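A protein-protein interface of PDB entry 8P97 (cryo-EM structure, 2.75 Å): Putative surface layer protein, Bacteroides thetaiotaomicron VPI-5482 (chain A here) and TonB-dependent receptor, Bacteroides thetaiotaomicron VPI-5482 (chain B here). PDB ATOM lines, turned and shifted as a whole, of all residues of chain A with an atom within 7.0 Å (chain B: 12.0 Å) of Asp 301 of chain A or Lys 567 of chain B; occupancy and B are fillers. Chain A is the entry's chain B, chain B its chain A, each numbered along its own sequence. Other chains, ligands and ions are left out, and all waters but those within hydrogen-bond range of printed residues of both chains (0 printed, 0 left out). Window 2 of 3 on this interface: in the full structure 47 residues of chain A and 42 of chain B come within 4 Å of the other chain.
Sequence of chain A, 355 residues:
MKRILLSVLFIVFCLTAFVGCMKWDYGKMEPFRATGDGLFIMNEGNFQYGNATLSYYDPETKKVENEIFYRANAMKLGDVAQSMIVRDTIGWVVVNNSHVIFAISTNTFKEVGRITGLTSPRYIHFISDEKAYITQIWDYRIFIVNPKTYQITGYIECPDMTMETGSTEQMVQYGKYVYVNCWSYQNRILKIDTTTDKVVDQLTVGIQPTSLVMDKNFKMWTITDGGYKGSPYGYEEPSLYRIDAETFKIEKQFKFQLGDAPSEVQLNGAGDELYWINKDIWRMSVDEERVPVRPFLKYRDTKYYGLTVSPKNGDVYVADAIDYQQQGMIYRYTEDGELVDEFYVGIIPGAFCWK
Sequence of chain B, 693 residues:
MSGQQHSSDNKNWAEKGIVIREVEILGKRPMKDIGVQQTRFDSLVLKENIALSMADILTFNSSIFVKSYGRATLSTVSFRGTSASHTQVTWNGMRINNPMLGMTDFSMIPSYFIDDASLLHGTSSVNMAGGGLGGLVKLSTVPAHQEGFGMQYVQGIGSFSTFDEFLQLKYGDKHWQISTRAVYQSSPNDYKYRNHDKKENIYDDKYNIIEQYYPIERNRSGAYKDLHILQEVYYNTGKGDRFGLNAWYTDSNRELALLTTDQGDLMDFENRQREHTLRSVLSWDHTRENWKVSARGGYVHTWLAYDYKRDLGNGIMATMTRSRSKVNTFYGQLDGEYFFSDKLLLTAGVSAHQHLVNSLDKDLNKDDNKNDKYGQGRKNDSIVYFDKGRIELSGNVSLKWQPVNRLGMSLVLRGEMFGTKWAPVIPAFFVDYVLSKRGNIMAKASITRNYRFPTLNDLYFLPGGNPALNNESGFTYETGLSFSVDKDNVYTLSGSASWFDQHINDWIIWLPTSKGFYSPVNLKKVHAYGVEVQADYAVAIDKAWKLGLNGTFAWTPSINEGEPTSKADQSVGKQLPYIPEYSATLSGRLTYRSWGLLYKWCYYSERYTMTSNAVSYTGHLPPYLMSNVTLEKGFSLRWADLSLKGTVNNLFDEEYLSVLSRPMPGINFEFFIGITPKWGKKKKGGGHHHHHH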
ATOM      1  N   TYR A 299      19.240  -6.424  -5.985  1.00  0.00           N
ATOM      2  CA  TYR A 299      19.529  -7.572  -6.838  1.00  0.00           C
ATOM      3  C   TYR A 299      19.133  -8.856  -6.126  1.00  0.00           C
ATOM      4  O   TYR A 299      19.434  -9.029  -4.941  1.00  0.00           O
ATOM      5  CB  TYR A 299      21.008  -7.610  -7.228  1.00  0.00           C
ATOM      6  CG  TYR A 299      21.338  -8.609  -8.311  1.00  0.00           C
ATOM      7  CD1 TYR A 299      20.987  -8.364  -9.633  1.00  0.00           C
ATOM      8  CD2 TYR A 299      22.022  -9.781  -8.024  1.00  0.00           C
ATOM      9  CE1 TYR A 299      21.291  -9.264 -10.631  1.00  0.00           C
ATOM     10  CE2 TYR A 299      22.334 -10.686  -9.018  1.00  0.00           C
ATOM     11  CZ  TYR A 299      21.964 -10.424 -10.320  1.00  0.00           C
ATOM     12  OH  TYR A 299      22.270 -11.323 -11.313  1.00  0.00           O
ATOM     13  N   ARG A 300      18.474  -9.766  -6.832  1.00  0.00           N
ATOM     14  CA  ARG A 300      18.027 -11.020  -6.239  1.00  0.00           C
ATOM     15  C   ARG A 300      18.263 -12.156  -7.235  1.00  0.00           C
ATOM     16  O   ARG A 300      17.433 -13.046  -7.417  1.00  0.00           O
ATOM     17  CB  ARG A 300      16.567 -10.882  -5.798  1.00  0.00           C
ATOM     18  CG  ARG A 300      16.005 -12.007  -4.937  1.00  0.00           C
ATOM     19  CD  ARG A 300      14.930 -12.777  -5.680  1.00  0.00           C
ATOM     20  NE  ARG A 300      13.749 -11.955  -5.911  1.00  0.00           N
ATOM     21  CZ  ARG A 300      12.815 -12.224  -6.811  1.00  0.00           C
ATOM     22  NH1 ARG A 300      12.894 -13.288  -7.593  1.00  0.00           N
ATOM     23  NH2 ARG A 300      11.776 -11.403  -6.932  1.00  0.00           N
ATOM     24  N   ASP A 301      19.430 -12.127  -7.875  1.00  0.00           N
ATOM     25  CA  ASP A 301      19.838 -13.071  -8.921  1.00  0.00           C
ATOM     26  C   ASP A 301      18.682 -13.399  -9.868  1.00  0.00           C
ATOM     27  O   ASP A 301      18.245 -14.541 -10.005  1.00  0.00           O
ATOM     28  CB  ASP A 301      20.458 -14.344  -8.332  1.00  0.00           C
ATOM     29  CG  ASP A 301      19.569 -15.033  -7.314  1.00  0.00           C
ATOM     30  OD1 ASP A 301      19.493 -14.556  -6.163  1.00  0.00           O
ATOM     31  OD2 ASP A 301      18.946 -16.056  -7.666  1.00  0.00           O
ATOM     32  N   THR A 302      18.185 -12.350 -10.524  1.00  0.00           N
ATOM     33  CA  THR A 302      17.143 -12.465 -11.534  1.00  0.00           C
ATOM     34  C   THR A 302      17.563 -11.725 -12.795  1.00  0.00           C
ATOM     35  O   THR A 302      18.385 -10.805 -12.750  1.00  0.00           O
ATOM     36  CB  THR A 302      15.801 -11.907 -11.045  1.00  0.00           C
ATOM     37  OG1 THR A 302      15.923 -10.496 -10.843  1.00  0.00           O
ATOM     38  CG2 THR A 302      15.367 -12.573  -9.754  1.00  0.00           C
ATOM     39  N   LYS A 303      16.983 -12.133 -13.924  1.00  0.00           N
ATOM     40  CA  LYS A 303      17.293 -11.542 -15.224  1.00  0.00           C
ATOM     41  C   LYS A 303      16.099 -10.707 -15.680  1.00  0.00           C
ATOM     42  O   LYS A 303      15.188 -11.181 -16.358  1.00  0.00           O
ATOM     43  CB  LYS A 303      17.646 -12.630 -16.232  1.00  0.00           C
ATOM     44  CG  LYS A 303      18.856 -13.490 -15.860  1.00  0.00           C
ATOM     45  CD  LYS A 303      20.184 -12.737 -15.972  1.00  0.00           C
ATOM     46  CE  LYS A 303      20.635 -12.149 -14.641  1.00  0.00           C
ATOM     47  NZ  LYS A 303      21.977 -11.513 -14.739  1.00  0.00           N
ATOM     48  N   TYR A 304      16.122  -9.432 -15.301  1.00  0.00           N
ATOM     49  CA  TYR A 304      15.017  -8.529 -15.598  1.00  0.00           C
ATOM     50  C   TYR A 304      15.073  -8.096 -17.058  1.00  0.00           C
ATOM     51  O   TYR A 304      16.086  -7.560 -17.514  1.00  0.00           O
ATOM     52  CB  TYR A 304      15.084  -7.317 -14.675  1.00  0.00           C
ATOM     53  CG  TYR A 304      14.735  -7.639 -13.245  1.00  0.00           C
ATOM     54  CD1 TYR A 304      13.759  -8.575 -12.946  1.00  0.00           C
ATOM     55  CD2 TYR A 304      15.400  -7.029 -12.194  1.00  0.00           C
ATOM     56  CE1 TYR A 304      13.438  -8.876 -11.643  1.00  0.00           C
ATOM     57  CE2 TYR A 304      15.089  -7.326 -10.886  1.00  0.00           C
ATOM     58  CZ  TYR A 304      14.105  -8.249 -10.615  1.00  0.00           C
ATOM     59  OH  TYR A 304      13.789  -8.557  -9.313  1.00  0.00           O
ATOM     60  N   ASP A 320      10.486 -11.268 -15.823  1.00  0.00           N
ATOM     61  CA  ASP A 320      11.642 -12.158 -15.758  1.00  0.00           C
ATOM     62  C   ASP A 320      11.510 -13.187 -16.870  1.00  0.00           C
ATOM     63  O   ASP A 320      10.550 -13.962 -16.888  1.00  0.00           O
ATOM     64  CB  ASP A 320      11.738 -12.837 -14.393  1.00  0.00           C
ATOM     65  CG  ASP A 320      12.990 -13.668 -14.246  1.00  0.00           C
ATOM     66  OD1 ASP A 320      14.025 -13.297 -14.836  1.00  0.00           O
ATOM     67  OD2 ASP A 320      12.944 -14.693 -13.535  1.00  0.00           O
ATOM     68  N   ILE A 322      13.782 -15.583 -17.533  1.00  0.00           N
ATOM     69  CA  ILE A 322      14.450 -16.819 -17.134  1.00  0.00           C
ATOM     70  C   ILE A 322      15.530 -17.185 -18.147  1.00  0.00           C
ATOM     71  O   ILE A 322      16.647 -16.662 -18.087  1.00  0.00           O
ATOM     72  CB  ILE A 322      13.435 -17.962 -16.949  1.00  0.00           C
ATOM     73  CG1 ILE A 322      12.362 -17.546 -15.948  1.00  0.00           C
ATOM     74  CG2 ILE A 322      14.117 -19.206 -16.410  1.00  0.00           C
ATOM     75  CD1 ILE A 322      11.201 -18.496 -15.883  1.00  0.00           C
ATOM     76  N   MET A 329       7.992 -15.027 -15.803  1.00  0.00           N
ATOM     77  CA  MET A 329       7.210 -14.620 -14.646  1.00  0.00           C
ATOM     78  C   MET A 329       7.322 -13.120 -14.451  1.00  0.00           C
ATOM     79  O   MET A 329       8.393 -12.537 -14.643  1.00  0.00           O
ATOM     80  CB  MET A 329       7.652 -15.341 -13.366  1.00  0.00           C
ATOM     81  CG  MET A 329       6.556 -15.385 -12.311  1.00  0.00           C
ATOM     82  SD  MET A 329       6.792 -16.536 -10.946  1.00  0.00           S
ATOM     83  CE  MET A 329       8.470 -16.174 -10.474  1.00  0.00           C
ATOM     84  N   TYR A 331       6.797 -10.144 -11.578  1.00  0.00           N
ATOM     85  CA  TYR A 331       6.677  -9.832 -10.164  1.00  0.00           C
ATOM     86  C   TYR A 331       5.987  -8.487 -10.003  1.00  0.00           C
ATOM     87  O   TYR A 331       6.277  -7.539 -10.739  1.00  0.00           O
ATOM     88  CB  TYR A 331       8.047  -9.793  -9.493  1.00  0.00           C
ATOM     89  CG  TYR A 331       8.848 -11.064  -9.627  1.00  0.00           C
ATOM     90  CD1 TYR A 331       8.773 -12.057  -8.666  1.00  0.00           C
ATOM     91  CD2 TYR A 331       9.688 -11.263 -10.710  1.00  0.00           C
ATOM     92  CE1 TYR A 331       9.507 -13.213  -8.782  1.00  0.00           C
ATOM     93  CE2 TYR A 331      10.424 -12.416 -10.835  1.00  0.00           C
ATOM     94  CZ  TYR A 331      10.331 -13.387  -9.869  1.00  0.00           C
ATOM     95  OH  TYR A 331      11.070 -14.539  -9.993  1.00  0.00           O
ATOM     96  N   TYR A 344       2.644 -16.408 -14.234  1.00  0.00           N
ATOM     97  CA  TYR A 344       3.278 -16.908 -15.444  1.00  0.00           C
ATOM     98  C   TYR A 344       2.573 -16.406 -16.696  1.00  0.00           C
ATOM     99  O   TYR A 344       1.348 -16.269 -16.736  1.00  0.00           O
ATOM    100  CB  TYR A 344       3.284 -18.435 -15.439  1.00  0.00           C
ATOM    101  CG  TYR A 344       4.330 -19.044 -14.542  1.00  0.00           C
ATOM    102  CD1 TYR A 344       5.455 -18.328 -14.170  1.00  0.00           C
ATOM    103  CD2 TYR A 344       4.169 -20.319 -14.030  1.00  0.00           C
ATOM    104  CE1 TYR A 344       6.409 -18.881 -13.349  1.00  0.00           C
ATOM    105  CE2 TYR A 344       5.111 -20.873 -13.196  1.00  0.00           C
ATOM    106  CZ  TYR A 344       6.232 -20.152 -12.860  1.00  0.00           C
ATOM    107  OH  TYR A 344       7.177 -20.703 -12.032  1.00  0.00           O
ATOM    108  N   LEU B 511      23.098 -17.962 -23.944  1.00  0.00           N
ATOM    109  CA  LEU B 511      21.977 -17.295 -23.321  1.00  0.00           C
ATOM    110  C   LEU B 511      22.488 -15.959 -22.792  1.00  0.00           C
ATOM    111  O   LEU B 511      23.536 -15.919 -22.122  1.00  0.00           O
ATOM    112  CB  LEU B 511      21.349 -18.139 -22.203  1.00  0.00           C
ATOM    113  CG  LEU B 511      22.145 -18.584 -20.969  1.00  0.00           C
ATOM    114  CD1 LEU B 511      22.152 -17.535 -19.861  1.00  0.00           C
ATOM    115  CD2 LEU B 511      21.607 -19.908 -20.447  1.00  0.00           C
ATOM    116  N   PRO B 512      21.810 -14.849 -23.109  1.00  0.00           N
ATOM    117  CA  PRO B 512      22.168 -13.511 -22.626  1.00  0.00           C
ATOM    118  C   PRO B 512      22.189 -13.416 -21.103  1.00  0.00           C
ATOM    119  O   PRO B 512      22.229 -12.306 -20.574  1.00  0.00           O
ATOM    120  CB  PRO B 512      21.061 -12.634 -23.207  1.00  0.00           C
ATOM    121  CG  PRO B 512      20.690 -13.324 -24.469  1.00  0.00           C
ATOM    122  CD  PRO B 512      20.778 -14.792 -24.158  1.00  0.00           C
ATOM    123  N   LEU B 523      27.811 -24.619 -18.304  1.00  0.00           N
ATOM    124  CA  LEU B 523      26.765 -25.196 -17.463  1.00  0.00           C
ATOM    125  C   LEU B 523      25.963 -26.251 -18.218  1.00  0.00           C
ATOM    126  O   LEU B 523      26.506 -26.951 -19.077  1.00  0.00           O
ATOM    127  CB  LEU B 523      25.835 -24.105 -16.928  1.00  0.00           C
ATOM    128  CG  LEU B 523      26.455 -23.096 -15.958  1.00  0.00           C
ATOM    129  CD1 LEU B 523      25.457 -21.999 -15.625  1.00  0.00           C
ATOM    130  CD2 LEU B 523      26.940 -23.787 -14.694  1.00  0.00           C
ATOM    131  N   GLY B 562      21.051 -29.695 -14.276  1.00  0.00           N
ATOM    132  CA  GLY B 562      21.711 -28.479 -13.853  1.00  0.00           C
ATOM    133  C   GLY B 562      21.008 -27.817 -12.684  1.00  0.00           C
ATOM    134  O   GLY B 562      19.823 -28.028 -12.434  1.00  0.00           O
ATOM    135  N   GLU B 563      21.769 -27.015 -11.950  1.00  0.00           N
ATOM    136  CA  GLU B 563      21.204 -26.271 -10.838  1.00  0.00           C
ATOM    137  C   GLU B 563      20.203 -25.244 -11.364  1.00  0.00           C
ATOM    138  O   GLU B 563      20.465 -24.587 -12.379  1.00  0.00           O
ATOM    139  CB  GLU B 563      22.313 -25.580 -10.043  1.00  0.00           C
ATOM    140  CG  GLU B 563      21.869 -24.988  -8.716  1.00  0.00           C
ATOM    141  CD  GLU B 563      21.828 -26.013  -7.597  1.00  0.00           C
ATOM    142  OE1 GLU B 563      21.728 -27.223  -7.889  1.00  0.00           O
ATOM    143  OE2 GLU B 563      21.892 -25.605  -6.419  1.00  0.00           O
ATOM    144  N   PRO B 564      19.044 -25.090 -10.716  1.00  0.00           N
ATOM    145  CA  PRO B 564      18.021 -24.176 -11.238  1.00  0.00           C
ATOM    146  C   PRO B 564      18.502 -22.742 -11.361  1.00  0.00           C
ATOM    147  O   PRO B 564      18.805 -22.093 -10.356  1.00  0.00           O
ATOM    148  CB  PRO B 564      16.896 -24.286 -10.202  1.00  0.00           C
ATOM    149  CG  PRO B 564      17.086 -25.612  -9.577  1.00  0.00           C
ATOM    150  CD  PRO B 564      18.565 -25.848  -9.550  1.00  0.00           C
ATOM    151  N   THR B 565      18.580 -22.240 -12.589  1.00  0.00           N
ATOM    152  CA  THR B 565      18.829 -20.822 -12.795  1.00  0.00           C
ATOM    153  C   THR B 565      17.617 -20.024 -12.339  1.00  0.00           C
ATOM    154  O   THR B 565      16.474 -20.441 -12.539  1.00  0.00           O
ATOM    155  CB  THR B 565      19.126 -20.535 -14.265  1.00  0.00           C
ATOM    156  OG1 THR B 565      17.993 -20.899 -15.062  1.00  0.00           O
ATOM    157  CG2 THR B 565      20.337 -21.331 -14.723  1.00  0.00           C
ATOM    158  N   SER B 566      17.870 -18.874 -11.716  1.00  0.00           N
ATOM    159  CA  SER B 566      16.809 -18.072 -11.119  1.00  0.00           C
ATOM    160  C   SER B 566      16.007 -18.903 -10.126  1.00  0.00           C
ATOM    161  O   SER B 566      16.546 -19.820  -9.500  1.00  0.00           O
ATOM    162  CB  SER B 566      15.891 -17.488 -12.198  1.00  0.00           C
ATOM    163  OG  SER B 566      16.599 -16.597 -13.040  1.00  0.00           O
ATOM    164  N   LYS B 567      14.721 -18.594  -9.975  1.00  0.00           N
ATOM    165  CA  LYS B 567      13.871 -19.272  -9.004  1.00  0.00           C
ATOM    166  C   LYS B 567      12.616 -19.891  -9.593  1.00  0.00           C
ATOM    167  O   LYS B 567      12.055 -20.799  -8.970  1.00  0.00           O
ATOM    168  CB  LYS B 567      13.454 -18.305  -7.884  1.00  0.00           C
ATOM    169  CG  LYS B 567      14.479 -18.130  -6.772  1.00  0.00           C
ATOM    170  CD  LYS B 567      15.664 -17.298  -7.225  1.00  0.00           C
ATOM    171  CE  LYS B 567      15.275 -15.853  -7.453  1.00  0.00           C
ATOM    172  NZ  LYS B 567      16.452 -15.031  -7.838  1.00  0.00           N
ATOM    173  N   ALA B 568      12.154 -19.439 -10.756  1.00  0.00           N
ATOM    174  CA  ALA B 568      10.965 -19.978 -11.397  1.00  0.00           C
ATOM    175  C   ALA B 568      11.295 -20.981 -12.489  1.00  0.00           C
ATOM    176  O   ALA B 568      10.405 -21.364 -13.253  1.00  0.00           O
ATOM    177  CB  ALA B 568      10.121 -18.848 -11.978  1.00  0.00           C
ATOM    178  N   ASP B 569      12.548 -21.410 -12.584  1.00  0.00           N
ATOM    179  CA  ASP B 569      12.964 -22.338 -13.625  1.00  0.00           C
ATOM    180  C   ASP B 569      12.274 -23.677 -13.414  1.00  0.00           C
ATOM    181  O   ASP B 569      12.644 -24.438 -12.515  1.00  0.00           O
ATOM    182  CB  ASP B 569      14.480 -22.504 -13.597  1.00  0.00           C
ATOM    183  CG  ASP B 569      15.066 -22.749 -14.964  1.00  0.00           C
ATOM    184  OD1 ASP B 569      14.370 -23.340 -15.812  1.00  0.00           O
ATOM    185  OD2 ASP B 569      16.229 -22.358 -15.191  1.00  0.00           O
ATOM    186  N   GLN B 570      11.266 -23.966 -14.229  1.00  0.00           N
ATOM    187  CA  GLN B 570      10.615 -25.272 -14.190  1.00  0.00           C
ATOM    188  C   GLN B 570      11.239 -26.220 -15.203  1.00  0.00           C
ATOM    189  O   GLN B 570      10.541 -26.884 -15.966  1.00  0.00           O
ATOM    190  CB  GLN B 570       9.125 -25.116 -14.451  1.00  0.00           C
ATOM    191  CG  GLN B 570       8.477 -23.984 -13.704  1.00  0.00           C
ATOM    192  CD  GLN B 570       7.157 -23.599 -14.318  1.00  0.00           C
ATOM    193  OE1 GLN B 570       6.989 -22.484 -14.799  1.00  0.00           O
ATOM    194  NE2 GLN B 570       6.206 -24.523 -14.304  1.00  0.00           N
ATOM    195  N   SER B 571      12.565 -26.311 -15.207  1.00  0.00           N
ATOM    196  CA  SER B 571      13.261 -27.097 -16.211  1.00  0.00           C
ATOM    197  C   SER B 571      14.147 -28.189 -15.638  1.00  0.00           C
ATOM    198  O   SER B 571      14.669 -28.996 -16.410  1.00  0.00           O
ATOM    199  CB  SER B 571      14.109 -26.190 -17.114  1.00  0.00           C
ATOM    200  OG  SER B 571      15.074 -25.481 -16.362  1.00  0.00           O
ATOM    201  N   VAL B 572      14.328 -28.251 -14.321  1.00  0.00           N
ATOM    202  CA  VAL B 572      15.141 -29.308 -13.736  1.00  0.00           C
ATOM    203  C   VAL B 572      14.357 -30.611 -13.748  1.00  0.00           C
ATOM    204  O   VAL B 572      13.207 -30.667 -13.297  1.00  0.00           O
ATOM    205  CB  VAL B 572      15.578 -28.926 -12.316  1.00  0.00           C
ATOM    206  CG1 VAL B 572      16.218 -30.111 -11.624  1.00  0.00           C
ATOM    207  CG2 VAL B 572      16.541 -27.764 -12.371  1.00  0.00           C
ATOM    208  N   LYS B 574      13.612 -32.213 -16.632  1.00  0.00           N
ATOM    209  CA  LYS B 574      12.714 -32.083 -17.767  1.00  0.00           C
ATOM    210  C   LYS B 574      13.390 -32.540 -19.051  1.00  0.00           C
ATOM    211  O   LYS B 574      14.611 -32.448 -19.198  1.00  0.00           O
ATOM    212  CB  LYS B 574      12.245 -30.638 -17.923  1.00  0.00           C
ATOM    213  CG  LYS B 574      11.454 -30.106 -16.749  1.00  0.00           C
ATOM    214  CD  LYS B 574      10.176 -30.890 -16.539  1.00  0.00           C
ATOM    215  CE  LYS B 574       9.284 -30.204 -15.526  1.00  0.00           C
ATOM    216  NZ  LYS B 574       7.996 -30.923 -15.358  1.00  0.00           N
ATOM    217  N   THR B 611      11.581 -25.645 -22.567  1.00  0.00           N
ATOM    218  CA  THR B 611      12.374 -26.398 -21.603  1.00  0.00           C
ATOM    219  C   THR B 611      11.569 -26.805 -20.378  1.00  0.00           C
ATOM    220  O   THR B 611      11.992 -27.709 -19.652  1.00  0.00           O
ATOM    221  CB  THR B 611      13.593 -25.588 -21.168  1.00  0.00           C
ATOM    222  OG1 THR B 611      13.162 -24.403 -20.488  1.00  0.00           O
ATOM    223  CG2 THR B 611      14.424 -25.196 -22.367  1.00  0.00           C
ATOM    224  N   SER B 612      10.430 -26.162 -20.127  1.00  0.00           N
ATOM    225  CA  SER B 612       9.594 -26.520 -18.992  1.00  0.00           C
ATOM    226  C   SER B 612       8.574 -27.598 -19.323  1.00  0.00           C
ATOM    227  O   SER B 612       7.886 -28.072 -18.413  1.00  0.00           O
ATOM    228  CB  SER B 612       8.869 -25.284 -18.464  1.00  0.00           C
ATOM    229  OG  SER B 612       7.940 -24.799 -19.415  1.00  0.00           O
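The side-chain amino group (NZ) of Lys 567 of chain B lies within salt-bridge range of the side-chain carboxylate (OD2) of Asp 301 of chain A. OE1 of Gln 570 of chain B sits close to OH of Tyr 344 of chain A, at 3.3 Å. O of Arg 300 of chain A lies close to NZ of Lys 567 of chain B, 2.3 Å away.
NH1 of Arg 300 of chain A is in hydrogen-bond range of OH of Tyr 331 of chain A. The side-chain hydroxyl (OH) of Tyr 304 of chain A sits close to the side-chain hydroxyl (OG1) of Thr 302 of chain A. The backbone carbonyl oxygen of Met 329 of chain A sits at hydrogen-bond distance from the backbone NH of Asp 320 of chain A.
Ser 566 of chain B touches Asp 301 of chain A (CA to O, 3.97 Å). Lys 567 of chain B touches Thr 302 of chain A. Ala 568 of chain B touches Ile 322 of chain A. Ile 322 of chain A touches Asp 569 of chain B (CG2 to CG, 3.9 Å). Ala 568 of chain B touches Met 329 of chain A (CB to CE, 3.5 Å). Tyr 344 of chain A touches Ala 568 of chain B (OH to CB, 3.5 Å).
Lys 567 of chain B touches three residues of chain A. No residue of chain B comes within 4 Å of Tyr 299 of chain A. Arg 300 of chain A touches just one residue of chain B: Lys 567. Printed residues of chain B within 4 Å of Thr 302 of chain A: Lys 567. No residue of chain B comes within 4 Å of Lys 303 of chain A. Printed residues of chain A within 4 Å of Ser 566 of chain B: Asp 301 (3.97 Å). Printed residues of chain A within 4 Å of Asp 569 of chain B: Ile 322. Of the printed residues of chain B, Met 329 of chain A touches Ala 568. Tyr 304 of chain A touches none of the printed residues of chain B. Asp 320 of chain A touches none of the printed residues of chain B. The nearest residue of chain B that does not touch Asp 301 of chain A is Thr 565 of chain B (6.0 Å). The nearest residue of chain A that does not touch Lys 567 of chain B is Tyr 331 of chain A (4.9 Å). The nearest printed residue of chain A that does not touch Asp 569 of chain B is Tyr 344 of chain A (5.4 Å).
Of the 11 printed residues of chain A, 6 touch a printed residue of chain B. Printed residues of chain A that touch a printed residue of chain B: Arg 300, Asp 301, Thr 302, Ile 322, Met 329 and Tyr 344. Hydrophobic or aromatic side chains of chain A within 4 Å of the printed part of chain B: Ile 322, Met 329 and Tyr 344. Of the 17 printed residues of chain B, 5 touch a printed residue of chain A. Hydrophobic or aromatic side chains of chain B that line the printed part of chain A: Ala 568. Among the printed residues, Asp or Glu carboxylates within 4 Å of a Lys or Arg side-chain nitrogen of the other chain: Asp 301 of chain A with Lys 567 of chain B (2.7 Å).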
